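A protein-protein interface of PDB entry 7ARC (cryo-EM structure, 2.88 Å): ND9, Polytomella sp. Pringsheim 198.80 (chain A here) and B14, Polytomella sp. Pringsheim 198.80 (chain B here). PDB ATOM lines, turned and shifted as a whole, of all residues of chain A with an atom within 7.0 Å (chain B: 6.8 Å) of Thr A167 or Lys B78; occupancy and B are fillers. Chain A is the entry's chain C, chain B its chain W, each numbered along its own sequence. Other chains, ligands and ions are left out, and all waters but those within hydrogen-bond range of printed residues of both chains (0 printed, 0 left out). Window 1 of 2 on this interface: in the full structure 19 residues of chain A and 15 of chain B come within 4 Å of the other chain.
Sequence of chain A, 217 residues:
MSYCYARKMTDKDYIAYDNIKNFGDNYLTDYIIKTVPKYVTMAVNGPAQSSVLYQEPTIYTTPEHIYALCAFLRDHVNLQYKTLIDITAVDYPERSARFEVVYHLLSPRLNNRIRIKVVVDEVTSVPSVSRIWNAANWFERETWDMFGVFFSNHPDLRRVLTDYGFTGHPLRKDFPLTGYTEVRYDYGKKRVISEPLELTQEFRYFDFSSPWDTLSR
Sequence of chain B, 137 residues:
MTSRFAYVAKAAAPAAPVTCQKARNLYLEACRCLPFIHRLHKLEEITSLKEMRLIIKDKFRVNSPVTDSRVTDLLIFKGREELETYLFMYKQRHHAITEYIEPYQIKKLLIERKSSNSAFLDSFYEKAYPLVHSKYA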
ATOM      1  N   TRP A 144     -35.652 -16.415  -9.433  1.00  0.00           N
ATOM      2  CA  TRP A 144     -34.265 -16.803  -9.662  1.00  0.00           C
ATOM      3  C   TRP A 144     -34.145 -17.730 -10.862  1.00  0.00           C
ATOM      4  O   TRP A 144     -33.211 -17.607 -11.661  1.00  0.00           O
ATOM      5  CB  TRP A 144     -33.688 -17.468  -8.415  1.00  0.00           C
ATOM      6  CG  TRP A 144     -32.527 -18.362  -8.707  1.00  0.00           C
ATOM      7  CD1 TRP A 144     -32.497 -19.719  -8.612  1.00  0.00           C
ATOM      8  CD2 TRP A 144     -31.226 -17.964  -9.155  1.00  0.00           C
ATOM      9  NE1 TRP A 144     -31.262 -20.193  -8.969  1.00  0.00           N
ATOM     10  CE2 TRP A 144     -30.462 -19.134  -9.307  1.00  0.00           C
ATOM     11  CE3 TRP A 144     -30.633 -16.731  -9.439  1.00  0.00           C
ATOM     12  CZ2 TRP A 144     -29.138 -19.109  -9.731  1.00  0.00           C
ATOM     13  CZ3 TRP A 144     -29.320 -16.709  -9.859  1.00  0.00           C
ATOM     14  CH2 TRP A 144     -28.587 -17.888 -10.000  1.00  0.00           C
ATOM     15  N   ASP A 145     -35.079 -18.670 -11.002  1.00  0.00           N
ATOM     16  CA  ASP A 145     -35.016 -19.622 -12.105  1.00  0.00           C
ATOM     17  C   ASP A 145     -35.232 -18.928 -13.446  1.00  0.00           C
ATOM     18  O   ASP A 145     -34.451 -19.112 -14.386  1.00  0.00           O
ATOM     19  CB  ASP A 145     -36.058 -20.720 -11.888  1.00  0.00           C
ATOM     20  CG  ASP A 145     -35.892 -21.887 -12.834  1.00  0.00           C
ATOM     21  OD1 ASP A 145     -34.975 -21.858 -13.679  1.00  0.00           O
ATOM     22  OD2 ASP A 145     -36.685 -22.842 -12.730  1.00  0.00           O
ATOM     23  N   ARG A 159     -33.748 -23.878  -8.385  1.00  0.00           N
ATOM     24  CA  ARG A 159     -34.630 -23.773  -9.537  1.00  0.00           C
ATOM     25  C   ARG A 159     -35.868 -24.640  -9.332  1.00  0.00           C
ATOM     26  O   ARG A 159     -35.827 -25.672  -8.659  1.00  0.00           O
ATOM     27  CB  ARG A 159     -33.902 -24.194 -10.810  1.00  0.00           C
ATOM     28  CG  ARG A 159     -32.729 -23.312 -11.173  1.00  0.00           C
ATOM     29  CD  ARG A 159     -32.284 -23.575 -12.594  1.00  0.00           C
ATOM     30  NE  ARG A 159     -31.185 -22.705 -12.990  1.00  0.00           N
ATOM     31  CZ  ARG A 159     -31.229 -21.862 -14.011  1.00  0.00           C
ATOM     32  NH1 ARG A 159     -32.312 -21.736 -14.758  1.00  0.00           N
ATOM     33  NH2 ARG A 159     -30.158 -21.127 -14.289  1.00  0.00           N
ATOM     34  N   THR A 162     -37.615 -25.124 -14.519  1.00  0.00           N
ATOM     35  CA  THR A 162     -36.820 -25.617 -15.632  1.00  0.00           C
ATOM     36  C   THR A 162     -36.292 -27.024 -15.365  1.00  0.00           C
ATOM     37  O   THR A 162     -36.278 -27.514 -14.233  1.00  0.00           O
ATOM     38  CB  THR A 162     -35.657 -24.673 -15.925  1.00  0.00           C
ATOM     39  OG1 THR A 162     -34.878 -24.489 -14.736  1.00  0.00           O
ATOM     40  CG2 THR A 162     -36.172 -23.331 -16.413  1.00  0.00           C
ATOM     41  N   ASP A 163     -35.853 -27.669 -16.443  1.00  0.00           N
ATOM     42  CA  ASP A 163     -35.331 -29.026 -16.379  1.00  0.00           C
ATOM     43  C   ASP A 163     -34.073 -29.087 -15.520  1.00  0.00           C
ATOM     44  O   ASP A 163     -33.361 -28.096 -15.350  1.00  0.00           O
ATOM     45  CB  ASP A 163     -35.028 -29.530 -17.790  1.00  0.00           C
ATOM     46  CG  ASP A 163     -34.701 -31.002 -17.828  1.00  0.00           C
ATOM     47  OD1 ASP A 163     -35.033 -31.712 -16.857  1.00  0.00           O
ATOM     48  OD2 ASP A 163     -34.110 -31.452 -18.831  1.00  0.00           O
ATOM     49  N   TYR A 164     -33.814 -30.263 -14.954  1.00  0.00           N
ATOM     50  CA  TYR A 164     -32.585 -30.472 -14.199  1.00  0.00           C
ATOM     51  C   TYR A 164     -31.374 -30.290 -15.101  1.00  0.00           C
ATOM     52  O   TYR A 164     -31.328 -30.819 -16.215  1.00  0.00           O
ATOM     53  CB  TYR A 164     -32.575 -31.869 -13.587  1.00  0.00           C
ATOM     54  CG  TYR A 164     -33.690 -32.111 -12.603  1.00  0.00           C
ATOM     55  CD1 TYR A 164     -33.850 -31.297 -11.493  1.00  0.00           C
ATOM     56  CD2 TYR A 164     -34.586 -33.151 -12.787  1.00  0.00           C
ATOM     57  CE1 TYR A 164     -34.869 -31.513 -10.593  1.00  0.00           C
ATOM     58  CE2 TYR A 164     -35.606 -33.375 -11.894  1.00  0.00           C
ATOM     59  CZ  TYR A 164     -35.744 -32.554 -10.799  1.00  0.00           C
ATOM     60  OH  TYR A 164     -36.764 -32.776  -9.905  1.00  0.00           O
ATOM     61  N   GLY A 165     -30.390 -29.538 -14.617  1.00  0.00           N
ATOM     62  CA  GLY A 165     -29.222 -29.217 -15.405  1.00  0.00           C
ATOM     63  C   GLY A 165     -29.364 -27.995 -16.283  1.00  0.00           C
ATOM     64  O   GLY A 165     -28.410 -27.644 -16.987  1.00  0.00           O
ATOM     65  N   PHE A 166     -30.524 -27.344 -16.269  1.00  0.00           N
ATOM     66  CA  PHE A 166     -30.716 -26.122 -17.036  1.00  0.00           C
ATOM     67  C   PHE A 166     -29.928 -24.980 -16.413  1.00  0.00           C
ATOM     68  O   PHE A 166     -30.066 -24.695 -15.221  1.00  0.00           O
ATOM     69  CB  PHE A 166     -32.200 -25.769 -17.093  1.00  0.00           C
ATOM     70  CG  PHE A 166     -32.613 -25.087 -18.360  1.00  0.00           C
ATOM     71  CD1 PHE A 166     -32.809 -25.813 -19.519  1.00  0.00           C
ATOM     72  CD2 PHE A 166     -32.816 -23.720 -18.388  1.00  0.00           C
ATOM     73  CE1 PHE A 166     -33.192 -25.186 -20.682  1.00  0.00           C
ATOM     74  CE2 PHE A 166     -33.198 -23.091 -19.550  1.00  0.00           C
ATOM     75  CZ  PHE A 166     -33.387 -23.824 -20.697  1.00  0.00           C
ATOM     76  N   THR A 167     -29.086 -24.335 -17.218  1.00  0.00           N
ATOM     77  CA  THR A 167     -28.260 -23.238 -16.733  1.00  0.00           C
ATOM     78  C   THR A 167     -28.741 -21.870 -17.188  1.00  0.00           C
ATOM     79  O   THR A 167     -28.533 -20.890 -16.472  1.00  0.00           O
ATOM     80  CB  THR A 167     -26.806 -23.424 -17.183  1.00  0.00           C
ATOM     81  OG1 THR A 167     -26.728 -23.328 -18.609  1.00  0.00           O
ATOM     82  CG2 THR A 167     -26.287 -24.781 -16.747  1.00  0.00           C
ATOM     83  N   GLY A 168     -29.384 -21.782 -18.350  1.00  0.00           N
ATOM     84  CA  GLY A 168     -29.891 -20.513 -18.817  1.00  0.00           C
ATOM     85  C   GLY A 168     -31.164 -20.094 -18.113  1.00  0.00           C
ATOM     86  O   GLY A 168     -31.879 -20.898 -17.521  1.00  0.00           O
ATOM     87  N   HIS A 169     -31.439 -18.794 -18.171  1.00  0.00           N
ATOM     88  CA  HIS A 169     -32.653 -18.239 -17.597  1.00  0.00           C
ATOM     89  C   HIS A 169     -33.626 -17.897 -18.711  1.00  0.00           C
ATOM     90  O   HIS A 169     -33.370 -16.959 -19.478  1.00  0.00           O
ATOM     91  CB  HIS A 169     -32.325 -17.009 -16.761  1.00  0.00           C
ATOM     92  CG  HIS A 169     -31.186 -17.222 -15.816  1.00  0.00           C
ATOM     93  ND1 HIS A 169     -31.330 -17.877 -14.613  1.00  0.00           N
ATOM     94  CD2 HIS A 169     -29.876 -16.893 -15.910  1.00  0.00           C
ATOM     95  CE1 HIS A 169     -30.162 -17.931 -14.000  1.00  0.00           C
ATOM     96  NE2 HIS A 169     -29.263 -17.340 -14.765  1.00  0.00           N
ATOM     97  N   PHE A 175     -32.821 -14.645 -24.334  1.00  0.00           N
ATOM     98  CA  PHE A 175     -32.896 -16.096 -24.468  1.00  0.00           C
ATOM     99  C   PHE A 175     -33.769 -16.466 -25.664  1.00  0.00           C
ATOM    100  O   PHE A 175     -34.866 -15.921 -25.811  1.00  0.00           O
ATOM    101  CB  PHE A 175     -33.455 -16.719 -23.194  1.00  0.00           C
ATOM    102  CG  PHE A 175     -33.277 -18.205 -23.116  1.00  0.00           C
ATOM    103  CD1 PHE A 175     -32.075 -18.749 -22.715  1.00  0.00           C
ATOM    104  CD2 PHE A 175     -34.316 -19.057 -23.437  1.00  0.00           C
ATOM    105  CE1 PHE A 175     -31.913 -20.112 -22.641  1.00  0.00           C
ATOM    106  CE2 PHE A 175     -34.157 -20.421 -23.366  1.00  0.00           C
ATOM    107  CZ  PHE A 175     -32.955 -20.949 -22.967  1.00  0.00           C
ATOM    108  N   LEU B  26     -15.089 -24.698  -3.348  1.00  0.00           N
ATOM    109  CA  LEU B  26     -16.142 -25.420  -4.059  1.00  0.00           C
ATOM    110  C   LEU B  26     -15.598 -26.702  -4.681  1.00  0.00           C
ATOM    111  O   LEU B  26     -16.258 -27.751  -4.649  1.00  0.00           O
ATOM    112  CB  LEU B  26     -16.768 -24.525  -5.126  1.00  0.00           C
ATOM    113  CG  LEU B  26     -17.884 -25.157  -5.958  1.00  0.00           C
ATOM    114  CD1 LEU B  26     -19.069 -25.515  -5.080  1.00  0.00           C
ATOM    115  CD2 LEU B  26     -18.310 -24.224  -7.073  1.00  0.00           C
ATOM    116  N   ASP B  73     -19.286 -15.009  -7.634  1.00  0.00           N
ATOM    117  CA  ASP B  73     -20.224 -15.514  -6.638  1.00  0.00           C
ATOM    118  C   ASP B  73     -21.389 -16.229  -7.308  1.00  0.00           C
ATOM    119  O   ASP B  73     -21.796 -17.318  -6.883  1.00  0.00           O
ATOM    120  CB  ASP B  73     -20.723 -14.366  -5.764  1.00  0.00           C
ATOM    121  CG  ASP B  73     -19.637 -13.802  -4.868  1.00  0.00           C
ATOM    122  OD1 ASP B  73     -18.720 -14.560  -4.493  1.00  0.00           O
ATOM    123  OD2 ASP B  73     -19.702 -12.598  -4.538  1.00  0.00           O
ATOM    124  N   LEU B  74     -21.950 -15.617  -8.354  1.00  0.00           N
ATOM    125  CA  LEU B  74     -23.064 -16.245  -9.060  1.00  0.00           C
ATOM    126  C   LEU B  74     -22.638 -17.566  -9.685  1.00  0.00           C
ATOM    127  O   LEU B  74     -23.374 -18.561  -9.625  1.00  0.00           O
ATOM    128  CB  LEU B  74     -23.613 -15.308 -10.135  1.00  0.00           C
ATOM    129  CG  LEU B  74     -24.574 -14.206  -9.696  1.00  0.00           C
ATOM    130  CD1 LEU B  74     -24.774 -13.206 -10.818  1.00  0.00           C
ATOM    131  CD2 LEU B  74     -25.899 -14.805  -9.272  1.00  0.00           C
ATOM    132  N   LEU B  75     -21.451 -17.594 -10.297  1.00  0.00           N
ATOM    133  CA  LEU B  75     -20.966 -18.816 -10.927  1.00  0.00           C
ATOM    134  C   LEU B  75     -20.765 -19.919  -9.896  1.00  0.00           C
ATOM    135  O   LEU B  75     -21.086 -21.086 -10.152  1.00  0.00           O
ATOM    136  CB  LEU B  75     -19.662 -18.525 -11.667  1.00  0.00           C
ATOM    137  CG  LEU B  75     -19.804 -17.809 -13.008  1.00  0.00           C
ATOM    138  CD1 LEU B  75     -18.442 -17.531 -13.608  1.00  0.00           C
ATOM    139  CD2 LEU B  75     -20.651 -18.627 -13.964  1.00  0.00           C
ATOM    140  N   ILE B  76     -20.232 -19.568  -8.725  1.00  0.00           N
ATOM    141  CA  ILE B  76     -20.025 -20.555  -7.672  1.00  0.00           C
ATOM    142  C   ILE B  76     -21.357 -21.083  -7.165  1.00  0.00           C
ATOM    143  O   ILE B  76     -21.506 -22.283  -6.911  1.00  0.00           O
ATOM    144  CB  ILE B  76     -19.175 -19.957  -6.541  1.00  0.00           C
ATOM    145  CG1 ILE B  76     -17.770 -19.673  -7.057  1.00  0.00           C
ATOM    146  CG2 ILE B  76     -19.116 -20.898  -5.356  1.00  0.00           C
ATOM    147  CD1 ILE B  76     -16.988 -18.782  -6.171  1.00  0.00           C
ATOM    148  N   PHE B  77     -22.338 -20.198  -6.987  1.00  0.00           N
ATOM    149  CA  PHE B  77     -23.657 -20.638  -6.545  1.00  0.00           C
ATOM    150  C   PHE B  77     -24.279 -21.599  -7.554  1.00  0.00           C
ATOM    151  O   PHE B  77     -24.863 -22.623  -7.177  1.00  0.00           O
ATOM    152  CB  PHE B  77     -24.552 -19.420  -6.319  1.00  0.00           C
ATOM    153  CG  PHE B  77     -25.952 -19.760  -5.913  1.00  0.00           C
ATOM    154  CD1 PHE B  77     -26.224 -20.211  -4.636  1.00  0.00           C
ATOM    155  CD2 PHE B  77     -27.000 -19.613  -6.802  1.00  0.00           C
ATOM    156  CE1 PHE B  77     -27.511 -20.519  -4.257  1.00  0.00           C
ATOM    157  CE2 PHE B  77     -28.288 -19.921  -6.429  1.00  0.00           C
ATOM    158  CZ  PHE B  77     -28.544 -20.374  -5.155  1.00  0.00           C
ATOM    159  N   LYS B  78     -24.139 -21.298  -8.845  1.00  0.00           N
ATOM    160  CA  LYS B  78     -24.699 -22.175  -9.868  1.00  0.00           C
ATOM    161  C   LYS B  78     -23.976 -23.520  -9.905  1.00  0.00           C
ATOM    162  O   LYS B  78     -24.611 -24.568 -10.084  1.00  0.00           O
ATOM    163  CB  LYS B  78     -24.665 -21.480 -11.228  1.00  0.00           C
ATOM    164  CG  LYS B  78     -25.634 -20.309 -11.310  1.00  0.00           C
ATOM    165  CD  LYS B  78     -25.504 -19.529 -12.603  1.00  0.00           C
ATOM    166  CE  LYS B  78     -26.028 -20.330 -13.778  1.00  0.00           C
ATOM    167  NZ  LYS B  78     -26.017 -19.539 -15.037  1.00  0.00           N
ATOM    168  N   GLY B  79     -22.652 -23.516  -9.742  1.00  0.00           N
ATOM    169  CA  GLY B  79     -21.924 -24.774  -9.674  1.00  0.00           C
ATOM    170  C   GLY B  79     -22.304 -25.604  -8.461  1.00  0.00           C
ATOM    171  O   GLY B  79     -22.387 -26.835  -8.533  1.00  0.00           O
ATOM    172  N   ARG B  80     -22.531 -24.943  -7.325  1.00  0.00           N
ATOM    173  CA  ARG B  80     -23.033 -25.645  -6.151  1.00  0.00           C
ATOM    174  C   ARG B  80     -24.393 -26.266  -6.431  1.00  0.00           C
ATOM    175  O   ARG B  80     -24.678 -27.380  -5.980  1.00  0.00           O
ATOM    176  CB  ARG B  80     -23.117 -24.696  -4.959  1.00  0.00           C
ATOM    177  CG  ARG B  80     -23.060 -25.394  -3.616  1.00  0.00           C
ATOM    178  CD  ARG B  80     -22.703 -24.425  -2.507  1.00  0.00           C
ATOM    179  NE  ARG B  80     -21.487 -23.674  -2.792  1.00  0.00           N
ATOM    180  CZ  ARG B  80     -20.424 -23.649  -2.001  1.00  0.00           C
ATOM    181  NH1 ARG B  80     -20.397 -24.316  -0.860  1.00  0.00           N
ATOM    182  NH2 ARG B  80     -19.365 -22.927  -2.358  1.00  0.00           N
ATOM    183  N   GLU B  81     -25.250 -25.556  -7.168  1.00  0.00           N
ATOM    184  CA  GLU B  81     -26.529 -26.137  -7.567  1.00  0.00           C
ATOM    185  C   GLU B  81     -26.325 -27.376  -8.429  1.00  0.00           C
ATOM    186  O   GLU B  81     -27.018 -28.388  -8.257  1.00  0.00           O
ATOM    187  CB  GLU B  81     -27.367 -25.108  -8.322  1.00  0.00           C
ATOM    188  CG  GLU B  81     -28.277 -24.265  -7.454  1.00  0.00           C
ATOM    189  CD  GLU B  81     -29.299 -23.503  -8.272  1.00  0.00           C
ATOM    190  OE1 GLU B  81     -28.917 -22.527  -8.950  1.00  0.00           O
ATOM    191  OE2 GLU B  81     -30.487 -23.886  -8.245  1.00  0.00           O
ATOM    192  N   GLU B  82     -25.380 -27.309  -9.368  1.00  0.00           N
ATOM    193  CA  GLU B  82     -25.105 -28.460 -10.225  1.00  0.00           C
ATOM    194  C   GLU B  82     -24.659 -29.658  -9.399  1.00  0.00           C
ATOM    195  O   GLU B  82     -25.070 -30.793  -9.665  1.00  0.00           O
ATOM    196  CB  GLU B  82     -24.044 -28.113 -11.269  1.00  0.00           C
ATOM    197  CG  GLU B  82     -24.427 -26.981 -12.205  1.00  0.00           C
ATOM    198  CD  GLU B  82     -23.221 -26.233 -12.742  1.00  0.00           C
ATOM    199  OE1 GLU B  82     -22.131 -26.836 -12.819  1.00  0.00           O
ATOM    200  OE2 GLU B  82     -23.365 -25.044 -13.095  1.00  0.00           O
ATOM    201  N   LEU B  83     -23.807 -29.427  -8.401  1.00  0.00           N
ATOM    202  CA  LEU B  83     -23.395 -30.518  -7.521  1.00  0.00           C
ATOM    203  C   LEU B  83     -24.576 -31.059  -6.716  1.00  0.00           C
ATOM    204  O   LEU B  83     -24.738 -32.279  -6.574  1.00  0.00           O
ATOM    205  CB  LEU B  83     -22.282 -30.043  -6.590  1.00  0.00           C
ATOM    206  CG  LEU B  83     -21.659 -31.075  -5.652  1.00  0.00           C
ATOM    207  CD1 LEU B  83     -20.778 -32.037  -6.425  1.00  0.00           C
ATOM    208  CD2 LEU B  83     -20.868 -30.382  -4.560  1.00  0.00           C
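The side-chain carboxylate (OE1) of Glu B81 is in hydrogen-bond range of the indole nitrogen (NE1) of Trp A144. OE2 of Glu B81 is in hydrogen-bond range of N of Arg A159, 3.3 Å away. The backbone carbonyl oxygen (O) of Thr A167 sits at hydrogen-bond distance from the side-chain amino group (NZ) of Lys B78 (3.2 Å).
Printed residues of chain B that touch a printed residue of chain A: Leu B74, Phe B77, Lys B78 and Glu B81. Of the 12 printed residues of chain A, 4 touch a printed residue of chain B. Printed residues of chain A that touch a printed residue of chain B: Trp A144, Arg A159, Thr A167 and His A169.
The side-chain carboxylate (OD1) of Asp A145 is in salt-bridge range of the guanidinium group (NH1) of Arg A159 (2.9 Å). The backbone carbonyl oxygen (O) of Gly A168 sits at hydrogen-bond distance from the guanidinium group (NH1) of Arg A159. The guanidinium group (NH2) of Arg A159 sits at hydrogen-bond distance from the backbone carbonyl oxygen (O) of Thr A167 (2.7 Å). The backbone carbonyl oxygen of Asp A145 lies within hydrogen-bond range of a ring nitrogen (ND1) of His A169. NH2 of Arg A159 lies close to ND1 of His A169, at 3.5 Å. The backbone carbonyl oxygen of Phe A166 sits at hydrogen-bond distance from the guanidinium group of Arg A159 (3.2 Å).
Among the printed residues, merely in contact across the chains: Trp A144 with Leu B74, Trp A144 with Phe B77 and His A169 with Lys B78.
Of the printed residues of chain B, Trp A144 touches Leu B74 (3.96 Å), Phe B77 (3.5 Å) and Glu B81 (3.3 Å). Of the printed residues of chain B, Arg A159 touches Glu B81 (3.3 Å). Thr A167 touches just one residue of chain B: Lys B78 (3.2 Å). Printed residues of chain B within 4 Å of His A169: Lys B78. Asp B73 touches none of the printed residues of chain A. Ile B76 touches none of the printed residues of chain A. Of chain A, only Thr A167 and His A169 come within 4 Å of Lys B78. Of the printed residues of chain A, Glu B81 touches Trp A144 and Arg A159. The nearest printed residue of chain B that does not touch Arg A159 is Lys B78 (4.2 Å).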
